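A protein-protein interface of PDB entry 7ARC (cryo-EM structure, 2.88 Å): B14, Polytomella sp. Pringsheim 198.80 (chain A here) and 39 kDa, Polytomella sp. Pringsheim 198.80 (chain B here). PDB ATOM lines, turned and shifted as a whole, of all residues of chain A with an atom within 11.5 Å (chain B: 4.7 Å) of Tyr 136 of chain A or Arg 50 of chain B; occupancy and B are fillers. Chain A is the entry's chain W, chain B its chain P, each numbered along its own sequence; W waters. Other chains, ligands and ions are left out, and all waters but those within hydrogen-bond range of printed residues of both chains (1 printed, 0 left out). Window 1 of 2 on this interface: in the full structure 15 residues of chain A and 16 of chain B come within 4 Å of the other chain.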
ATOM      1  N   THR A  98      -2.045  -7.788 -28.729  1.00  0.00           N
ATOM      2  CA  THR A  98      -2.202  -6.381 -28.388  1.00  0.00           C
ATOM      3  C   THR A  98      -1.994  -6.138 -26.902  1.00  0.00           C
ATOM      4  O   THR A  98      -1.343  -5.160 -26.516  1.00  0.00           O
ATOM      5  CB  THR A  98      -3.586  -5.890 -28.817  1.00  0.00           C
ATOM      6  OG1 THR A  98      -3.738  -6.049 -30.233  1.00  0.00           O
ATOM      7  CG2 THR A  98      -3.772  -4.425 -28.457  1.00  0.00           C
ATOM      8  N   GLU A 102       2.852  -7.515 -27.172  1.00  0.00           N
ATOM      9  CA  GLU A 102       3.387  -6.307 -27.796  1.00  0.00           C
ATOM     10  C   GLU A 102       3.924  -5.303 -26.785  1.00  0.00           C
ATOM     11  O   GLU A 102       5.028  -4.780 -27.009  1.00  0.00           O
ATOM     12  CB  GLU A 102       2.352  -5.657 -28.714  1.00  0.00           C
ATOM     13  CG  GLU A 102       2.945  -4.459 -29.424  1.00  0.00           C
ATOM     14  CD  GLU A 102       1.998  -3.796 -30.383  1.00  0.00           C
ATOM     15  OE1 GLU A 102       0.843  -4.248 -30.488  1.00  0.00           O
ATOM     16  OE2 GLU A 102       2.425  -2.829 -31.047  1.00  0.00           O
ATOM     17  N   ILE A 106       7.776  -4.081 -26.675  1.00  0.00           N
ATOM     18  CA  ILE A 106       8.066  -2.662 -26.846  1.00  0.00           C
ATOM     19  C   ILE A 106       8.949  -2.177 -25.707  1.00  0.00           C
ATOM     20  O   ILE A 106       9.916  -1.434 -25.916  1.00  0.00           O
ATOM     21  CB  ILE A 106       6.757  -1.858 -26.936  1.00  0.00           C
ATOM     22  CG1 ILE A 106       6.206  -1.882 -28.362  1.00  0.00           C
ATOM     23  CG2 ILE A 106       6.966  -0.425 -26.471  1.00  0.00           C
ATOM     24  CD1 ILE A 106       4.750  -1.498 -28.453  1.00  0.00           C
ATOM     25  N   LEU A 110      12.733  -0.582 -25.972  1.00  0.00           N
ATOM     26  CA  LEU A 110      12.764   0.850 -25.701  1.00  0.00           C
ATOM     27  C   LEU A 110      14.156   1.308 -25.273  1.00  0.00           C
ATOM     28  O   LEU A 110      14.737   0.767 -24.327  1.00  0.00           O
ATOM     29  CB  LEU A 110      11.729   1.194 -24.629  1.00  0.00           C
ATOM     30  CG  LEU A 110      11.423   2.653 -24.273  1.00  0.00           C
ATOM     31  CD1 LEU A 110      10.004   2.768 -23.746  1.00  0.00           C
ATOM     32  CD2 LEU A 110      12.396   3.191 -23.235  1.00  0.00           C
ATOM     33  N   ARG A 113      16.755   8.237 -23.067  1.00  0.00           N
ATOM     34  CA  ARG A 113      17.828   9.018 -22.470  1.00  0.00           C
ATOM     35  C   ARG A 113      17.487   9.326 -21.017  1.00  0.00           C
ATOM     36  O   ARG A 113      16.396   9.820 -20.714  1.00  0.00           O
ATOM     37  CB  ARG A 113      18.071  10.306 -23.261  1.00  0.00           C
ATOM     38  CG  ARG A 113      16.914  11.299 -23.279  1.00  0.00           C
ATOM     39  CD  ARG A 113      17.020  12.266 -24.446  1.00  0.00           C
ATOM     40  NE  ARG A 113      15.760  12.956 -24.699  1.00  0.00           N
ATOM     41  CZ  ARG A 113      15.270  13.207 -25.905  1.00  0.00           C
ATOM     42  NH1 ARG A 113      15.919  12.856 -27.003  1.00  0.00           N
ATOM     43  NH2 ARG A 113      14.100  13.830 -26.014  1.00  0.00           N
ATOM     44  N   GLU A 126       5.897  18.974 -20.101  1.00  0.00           N
ATOM     45  CA  GLU A 126       4.993  18.211 -20.957  1.00  0.00           C
ATOM     46  C   GLU A 126       3.601  18.834 -21.009  1.00  0.00           C
ATOM     47  O   GLU A 126       3.137  19.255 -22.073  1.00  0.00           O
ATOM     48  CB  GLU A 126       4.929  16.763 -20.473  1.00  0.00           C
ATOM     49  CG  GLU A 126       3.837  15.926 -21.110  1.00  0.00           C
ATOM     50  CD  GLU A 126       3.510  14.687 -20.299  1.00  0.00           C
ATOM     51  OE1 GLU A 126       3.772  13.568 -20.788  1.00  0.00           O
ATOM     52  OE2 GLU A 126       2.995  14.829 -19.171  1.00  0.00           O
ATOM     53  N   LYS A 127       2.916  18.913 -19.870  1.00  0.00           N
ATOM     54  CA  LYS A 127       1.536  19.375 -19.871  1.00  0.00           C
ATOM     55  C   LYS A 127       1.207  20.071 -18.559  1.00  0.00           C
ATOM     56  O   LYS A 127       1.880  19.885 -17.544  1.00  0.00           O
ATOM     57  CB  LYS A 127       0.557  18.227 -20.130  1.00  0.00           C
ATOM     58  CG  LYS A 127       0.537  17.166 -19.060  1.00  0.00           C
ATOM     59  CD  LYS A 127      -0.480  16.104 -19.406  1.00  0.00           C
ATOM     60  CE  LYS A 127      -0.002  15.237 -20.540  1.00  0.00           C
ATOM     61  NZ  LYS A 127      -0.938  14.112 -20.797  1.00  0.00           N
ATOM     62  N   VAL A 132      -3.949  14.023 -16.555  1.00  0.00           N
ATOM     63  CA  VAL A 132      -4.394  13.599 -17.876  1.00  0.00           C
ATOM     64  C   VAL A 132      -3.336  12.710 -18.515  1.00  0.00           C
ATOM     65  O   VAL A 132      -2.134  13.003 -18.460  1.00  0.00           O
ATOM     66  CB  VAL A 132      -4.706  14.818 -18.761  1.00  0.00           C
ATOM     67  CG1 VAL A 132      -5.465  14.385 -20.003  1.00  0.00           C
ATOM     68  CG2 VAL A 132      -5.500  15.849 -17.981  1.00  0.00           C
ATOM     69  N   HIS A 133      -3.779  11.617 -19.129  1.00  0.00           N
ATOM     70  CA  HIS A 133      -2.862  10.663 -19.732  1.00  0.00           C
ATOM     71  C   HIS A 133      -2.235  11.234 -21.001  1.00  0.00           C
ATOM     72  O   HIS A 133      -2.717  12.209 -21.583  1.00  0.00           O
ATOM     73  CB  HIS A 133      -3.588   9.362 -20.064  1.00  0.00           C
ATOM     74  CG  HIS A 133      -4.572   9.490 -21.183  1.00  0.00           C
ATOM     75  ND1 HIS A 133      -5.866   9.923 -20.991  1.00  0.00           N
ATOM     76  CD2 HIS A 133      -4.450   9.250 -22.510  1.00  0.00           C
ATOM     77  CE1 HIS A 133      -6.499   9.940 -22.150  1.00  0.00           C
ATOM     78  NE2 HIS A 133      -5.662   9.538 -23.088  1.00  0.00           N
ATOM     79  N   SER A 134      -1.137  10.614 -21.421  1.00  0.00           N
ATOM     80  CA  SER A 134      -0.486  10.907 -22.690  1.00  0.00           C
ATOM     81  C   SER A 134      -0.494   9.671 -23.576  1.00  0.00           C
ATOM     82  O   SER A 134      -0.230   8.561 -23.105  1.00  0.00           O
ATOM     83  CB  SER A 134       0.955  11.375 -22.483  1.00  0.00           C
ATOM     84  OG  SER A 134       1.000  12.598 -21.777  1.00  0.00           O
ATOM     85  N   LYS A 135      -0.797   9.863 -24.856  1.00  0.00           N
ATOM     86  CA  LYS A 135      -0.798   8.764 -25.807  1.00  0.00           C
ATOM     87  C   LYS A 135       0.436   8.831 -26.694  1.00  0.00           C
ATOM     88  O   LYS A 135       0.924   9.914 -27.029  1.00  0.00           O
ATOM     89  CB  LYS A 135      -2.054   8.783 -26.679  1.00  0.00           C
ATOM     90  CG  LYS A 135      -3.337   8.478 -25.940  1.00  0.00           C
ATOM     91  CD  LYS A 135      -4.517   8.484 -26.889  1.00  0.00           C
ATOM     92  CE  LYS A 135      -5.812   8.203 -26.157  1.00  0.00           C
ATOM     93  NZ  LYS A 135      -6.972   8.215 -27.082  1.00  0.00           N
ATOM     94  N   TYR A 136       0.933   7.651 -27.071  1.00  0.00           N
ATOM     95  CA  TYR A 136       2.076   7.516 -27.976  1.00  0.00           C
ATOM     96  C   TYR A 136       3.301   8.237 -27.421  1.00  0.00           C
ATOM     97  O   TYR A 136       4.019   8.928 -28.146  1.00  0.00           O
ATOM     98  CB  TYR A 136       1.734   8.007 -29.384  1.00  0.00           C
ATOM     99  CG  TYR A 136       0.349   7.609 -29.827  1.00  0.00           C
ATOM    100  CD1 TYR A 136      -0.015   6.273 -29.907  1.00  0.00           C
ATOM    101  CD2 TYR A 136      -0.596   8.565 -30.159  1.00  0.00           C
ATOM    102  CE1 TYR A 136      -1.279   5.903 -30.306  1.00  0.00           C
ATOM    103  CE2 TYR A 136      -1.862   8.205 -30.558  1.00  0.00           C
ATOM    104  CZ  TYR A 136      -2.200   6.873 -30.629  1.00  0.00           C
ATOM    105  OH  TYR A 136      -3.463   6.511 -31.029  1.00  0.00           O
ATOM    106  N   ALA A 137       3.535   8.076 -26.124  1.00  0.00           N
ATOM    107  CA  ALA A 137       4.643   8.736 -25.446  1.00  0.00           C
ATOM    108  C   ALA A 137       5.989   8.280 -25.999  1.00  0.00           C
ATOM    109  O   ALA A 137       6.980   9.006 -25.917  1.00  0.00           O
ATOM    110  CB  ALA A 137       4.571   8.482 -23.952  1.00  0.00           C
ATOM    111  N   LEU B   4       5.639  12.719 -23.017  1.00  0.00           N
ATOM    112  CA  LEU B   4       5.425  13.094 -24.407  1.00  0.00           C
ATOM    113  C   LEU B   4       6.318  14.262 -24.795  1.00  0.00           C
ATOM    114  O   LEU B   4       6.408  15.259 -24.074  1.00  0.00           O
ATOM    115  CB  LEU B   4       3.958  13.463 -24.625  1.00  0.00           C
ATOM    116  CG  LEU B   4       3.376  13.322 -26.031  1.00  0.00           C
ATOM    117  CD1 LEU B   4       3.680  11.961 -26.613  1.00  0.00           C
ATOM    118  CD2 LEU B   4       1.881  13.580 -26.012  1.00  0.00           C
ATOM    119  N   PHE B   7       6.207  18.278 -30.759  1.00  0.00           N
ATOM    120  CA  PHE B   7       6.678  18.510 -32.118  1.00  0.00           C
ATOM    121  C   PHE B   7       7.396  19.856 -32.161  1.00  0.00           C
ATOM    122  O   PHE B   7       6.771  20.900 -31.955  1.00  0.00           O
ATOM    123  CB  PHE B   7       5.498  18.494 -33.083  1.00  0.00           C
ATOM    124  CG  PHE B   7       5.208  17.145 -33.673  1.00  0.00           C
ATOM    125  CD1 PHE B   7       6.151  16.476 -34.425  1.00  0.00           C
ATOM    126  CD2 PHE B   7       3.974  16.551 -33.475  1.00  0.00           C
ATOM    127  CE1 PHE B   7       5.872  15.236 -34.960  1.00  0.00           C
ATOM    128  CE2 PHE B   7       3.691  15.314 -34.011  1.00  0.00           C
ATOM    129  CZ  PHE B   7       4.641  14.656 -34.754  1.00  0.00           C
ATOM    130  N   GLY B  20      -2.631  14.100 -27.072  1.00  0.00           N
ATOM    131  CA  GLY B  20      -1.801  13.592 -28.142  1.00  0.00           C
ATOM    132  C   GLY B  20      -2.385  12.467 -28.963  1.00  0.00           C
ATOM    133  O   GLY B  20      -1.639  11.824 -29.707  1.00  0.00           O
ATOM    134  N   GLY B  21      -3.681  12.202 -28.851  1.00  0.00           N
ATOM    135  CA  GLY B  21      -4.313  11.117 -29.559  1.00  0.00           C
ATOM    136  C   GLY B  21      -4.965  11.555 -30.853  1.00  0.00           C
ATOM    137  O   GLY B  21      -4.671  12.620 -31.405  1.00  0.00           O
ATOM    138  N   SER B  24      -7.047  14.685 -30.348  1.00  0.00           N
ATOM    139  CA  SER B  24      -6.270  15.807 -29.849  1.00  0.00           C
ATOM    140  C   SER B  24      -5.844  16.722 -30.994  1.00  0.00           C
ATOM    141  O   SER B  24      -5.978  16.396 -32.175  1.00  0.00           O
ATOM    142  CB  SER B  24      -5.031  15.303 -29.121  1.00  0.00           C
ATOM    143  OG  SER B  24      -5.392  14.382 -28.118  1.00  0.00           O
ATOM    144  N   GLY B  26      -2.733  18.533 -32.682  1.00  0.00           N
ATOM    145  CA  GLY B  26      -1.307  18.719 -32.895  1.00  0.00           C
ATOM    146  C   GLY B  26      -1.104  19.860 -33.876  1.00  0.00           C
ATOM    147  O   GLY B  26      -1.874  20.014 -34.827  1.00  0.00           O
ATOM    148  N   GLU B  46       1.382   7.848 -38.887  1.00  0.00           N
ATOM    149  CA  GLU B  46       2.043   8.382 -37.699  1.00  0.00           C
ATOM    150  C   GLU B  46       1.670   9.836 -37.453  1.00  0.00           C
ATOM    151  O   GLU B  46       1.376  10.225 -36.317  1.00  0.00           O
ATOM    152  CB  GLU B  46       3.556   8.233 -37.804  1.00  0.00           C
ATOM    153  CG  GLU B  46       4.019   6.852 -38.166  1.00  0.00           C
ATOM    154  CD  GLU B  46       3.639   5.794 -37.140  1.00  0.00           C
ATOM    155  OE1 GLU B  46       3.289   6.153 -35.996  1.00  0.00           O
ATOM    156  OE2 GLU B  46       3.692   4.593 -37.483  1.00  0.00           O
ATOM    157  N   ILE B  47       1.699  10.666 -38.496  1.00  0.00           N
ATOM    158  CA  ILE B  47       1.408  12.080 -38.284  1.00  0.00           C
ATOM    159  C   ILE B  47      -0.049  12.282 -37.884  1.00  0.00           C
ATOM    160  O   ILE B  47      -0.351  13.049 -36.964  1.00  0.00           O
ATOM    161  CB  ILE B  47       1.776  12.898 -39.534  1.00  0.00           C
ATOM    162  CG1 ILE B  47       3.260  12.732 -39.855  1.00  0.00           C
ATOM    163  CG2 ILE B  47       1.439  14.360 -39.332  1.00  0.00           C
ATOM    164  CD1 ILE B  47       3.666  13.333 -41.173  1.00  0.00           C
ATOM    165  N   SER B  48      -0.976  11.588 -38.546  1.00  0.00           N
ATOM    166  CA  SER B  48      -2.394  11.813 -38.302  1.00  0.00           C
ATOM    167  C   SER B  48      -2.872  11.161 -37.011  1.00  0.00           C
ATOM    168  O   SER B  48      -3.840  11.632 -36.406  1.00  0.00           O
ATOM    169  CB  SER B  48      -3.208  11.298 -39.486  1.00  0.00           C
ATOM    170  OG  SER B  48      -4.592  11.478 -39.264  1.00  0.00           O
ATOM    171  N   LYS B  49      -2.221  10.074 -36.591  1.00  0.00           N
ATOM    172  CA  LYS B  49      -2.579   9.376 -35.365  1.00  0.00           C
ATOM    173  C   LYS B  49      -2.517  10.289 -34.150  1.00  0.00           C
ATOM    174  O   LYS B  49      -3.300  10.124 -33.209  1.00  0.00           O
ATOM    175  CB  LYS B  49      -1.646   8.180 -35.201  1.00  0.00           C
ATOM    176  CG  LYS B  49      -1.884   7.307 -34.008  1.00  0.00           C
ATOM    177  CD  LYS B  49      -0.960   6.112 -34.079  1.00  0.00           C
ATOM    178  CE  LYS B  49       0.466   6.523 -33.775  1.00  0.00           C
ATOM    179  NZ  LYS B  49       1.382   5.356 -33.723  1.00  0.00           N
ATOM    180  N   ARG B  50      -1.603  11.253 -34.155  1.00  0.00           N
ATOM    181  CA  ARG B  50      -1.375  12.135 -33.023  1.00  0.00           C
ATOM    182  C   ARG B  50      -2.186  13.420 -33.110  1.00  0.00           C
ATOM    183  O   ARG B  50      -1.825  14.416 -32.475  1.00  0.00           O
ATOM    184  CB  ARG B  50       0.117  12.444 -32.901  1.00  0.00           C
ATOM    185  CG  ARG B  50       0.966  11.191 -32.884  1.00  0.00           C
ATOM    186  CD  ARG B  50       2.443  11.497 -32.886  1.00  0.00           C
ATOM    187  NE  ARG B  50       3.194  10.432 -32.235  1.00  0.00           N
ATOM    188  CZ  ARG B  50       3.592   9.321 -32.839  1.00  0.00           C
ATOM    189  NH1 ARG B  50       3.323   9.093 -34.112  1.00  0.00           N
ATOM    190  NH2 ARG B  50       4.271   8.414 -32.145  1.00  0.00           N
ATOM    191  N   GLY B  51      -3.275  13.412 -33.872  1.00  0.00           N
ATOM    192  CA  GLY B  51      -4.164  14.549 -33.952  1.00  0.00           C
ATOM    193  C   GLY B  51      -3.775  15.618 -34.942  1.00  0.00           C
ATOM    194  O   GLY B  51      -4.397  16.685 -34.948  1.00  0.00           O
ATOM    195  N   ASN B  52      -2.774  15.377 -35.776  1.00  0.00           N
ATOM    196  CA  ASN B  52      -2.331  16.370 -36.740  1.00  0.00           C
ATOM    197  C   ASN B  52      -3.119  16.228 -38.037  1.00  0.00           C
ATOM    198  O   ASN B  52      -3.780  15.219 -38.284  1.00  0.00           O
ATOM    199  CB  ASN B  52      -0.837  16.223 -37.012  1.00  0.00           C
ATOM    200  CG  ASN B  52      -0.021  16.161 -35.742  1.00  0.00           C
ATOM    201  OD1 ASN B  52       0.351  17.185 -35.180  1.00  0.00           O
ATOM    202  ND2 ASN B  52       0.269  14.952 -35.287  1.00  0.00           N
ATOM    203  N   VAL B 226       8.973  10.329 -37.070  1.00  0.00           N
ATOM    204  CA  VAL B 226       8.382  11.073 -35.958  1.00  0.00           C
ATOM    205  C   VAL B 226       9.467  11.712 -35.098  1.00  0.00           C
ATOM    206  O   VAL B 226       9.341  12.865 -34.672  1.00  0.00           O
ATOM    207  CB  VAL B 226       7.462  10.166 -35.122  1.00  0.00           C
ATOM    208  CG1 VAL B 226       6.711  10.993 -34.107  1.00  0.00           C
ATOM    209  CG2 VAL B 226       6.479   9.453 -36.016  1.00  0.00           C
ATOM    210  N   LYS B 230      10.097  15.617 -34.178  1.00  0.00           N
ATOM    211  CA  LYS B 230      10.116  16.062 -32.788  1.00  0.00           C
ATOM    212  C   LYS B 230      11.442  16.669 -32.352  1.00  0.00           C
ATOM    213  O   LYS B 230      11.567  17.034 -31.180  1.00  0.00           O
ATOM    214  CB  LYS B 230       9.757  14.916 -31.838  1.00  0.00           C
ATOM    215  CG  LYS B 230       8.326  14.440 -31.934  1.00  0.00           C
ATOM    216  CD  LYS B 230       8.054  13.353 -30.912  1.00  0.00           C
ATOM    217  CE  LYS B 230       6.639  12.814 -31.037  1.00  0.00           C
ATOM    218  NZ  LYS B 230       5.619  13.827 -30.657  1.00  0.00           N
HETATM  219  O   HOH W   1       0.902  11.794 -29.036  1.00  0.00           O
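The backbone NH (N) of Leu 4 of chain B is in hydrogen-bond range of the side-chain carboxylate (OE1) of Glu 126 of chain A, 3.0 Å away.
The side-chain carboxylate of Glu 46 of chain B lies within salt-bridge range of the guanidinium group of Arg 50 of chain B, at 3.5 Å.
N of Gly 20 of chain B lies within hydrogen-bond range of OG of Ser 24 of chain B, 3.0 Å away.
The side-chain carboxylate of Glu 46 of chain B lies within salt-bridge range of the side-chain amino group of Lys 49 of chain B, at 3.1 Å.
OE1 of Glu 126 of chain A lies within hydrogen-bond range of OG of Ser 134 of chain A.
N of Gly 21 of chain B sits at hydrogen-bond distance from OG of Ser 24 of chain B, 2.9 Å away.
O of Gly 21 of chain B sits at hydrogen-bond distance from N of Gly 51 of chain B (2.9 Å).
Among the printed residues, pairs that only touch across the chains: Lys 135 of chain A with Leu 4 of chain B, Lys 135 of chain A with Gly 21 of chain B, Tyr 136 of chain A with Leu 4 of chain B, Tyr 136 of chain A with Gly 20 of chain B, Tyr 136 of chain A with Gly 21 of chain B, Tyr 136 of chain A with Lys 49 of chain B, Tyr 136 of chain A with Arg 50 of chain B and Ala 137 of chain A with Leu 4 of chain B.
Tyr 136 of chain A touches just these residues of chain B: Leu 4 (3.4 Å), Gly 20 (3.5 Å), Gly 21 (3.9 Å), Lys 49 (3.4 Å) and Arg 50 (3.8 Å).
Arg 50 of chain B touches one residue of chain A.
Gly 20 of chain B touches one residue of chain A.
Gly 21 of chain B touches just these residues of chain A: Lys 135 and Tyr 136.
No residue of chain A comes within 4 Å of Glu 46 of chain B.
Lys 49 of chain B touches just one residue of chain A: Tyr 136 (3.4 Å).
No residue of chain A comes within 4 Å of Gly 51 of chain B.
Asn 52 of chain B touches none of the printed residues of chain A.
No residue of chain A comes within 4 Å of Val 226 of chain B.
Printed residues of chain B within 4 Å of Ala 137 of chain A: Leu 4.
Printed residues of chain A within 4 Å of Leu 4 of chain B: Glu 126, Lys 135, Tyr 136 and Ala 137.
Printed residues of chain B within 4 Å of Glu 126 of chain A: Leu 4 (3.0 Å).
Of the printed residues of chain B, Lys 135 of chain A touches Leu 4 and Gly 21.
The nearest printed residue of chain B that does not touch Tyr 136 of chain A is Lys 230 of chain B (5.5 Å).
The nearest residue of chain A that does not touch Arg 50 of chain B is Lys 135 of chain A (5.7 Å).
The nearest printed residue of chain B that does not touch Glu 126 of chain A is Gly 20 of chain B (9.0 Å).
Of the 13 printed residues of chain A, 4 touch a printed residue of chain B.
Hydrophobic or aromatic side chains of chain A within 4 Å of the printed part of chain B: Tyr 136.
Of the 15 printed residues of chain B, 5 touch a printed residue of chain A.
Hydrophobic or aromatic side chains of chain B within 4 Å of the printed part of chain A: Leu 4.
Among the printed residues, 9 pairs touch across the chains.
Among the printed residues, no Asp or Glu carboxylate lies within 4 Å of a Lys or Arg side-chain nitrogen of the other chain.
Water W1 lies within hydrogen-bond range of O of Gly 20 of chain B and O of Lys 135 of chain A.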
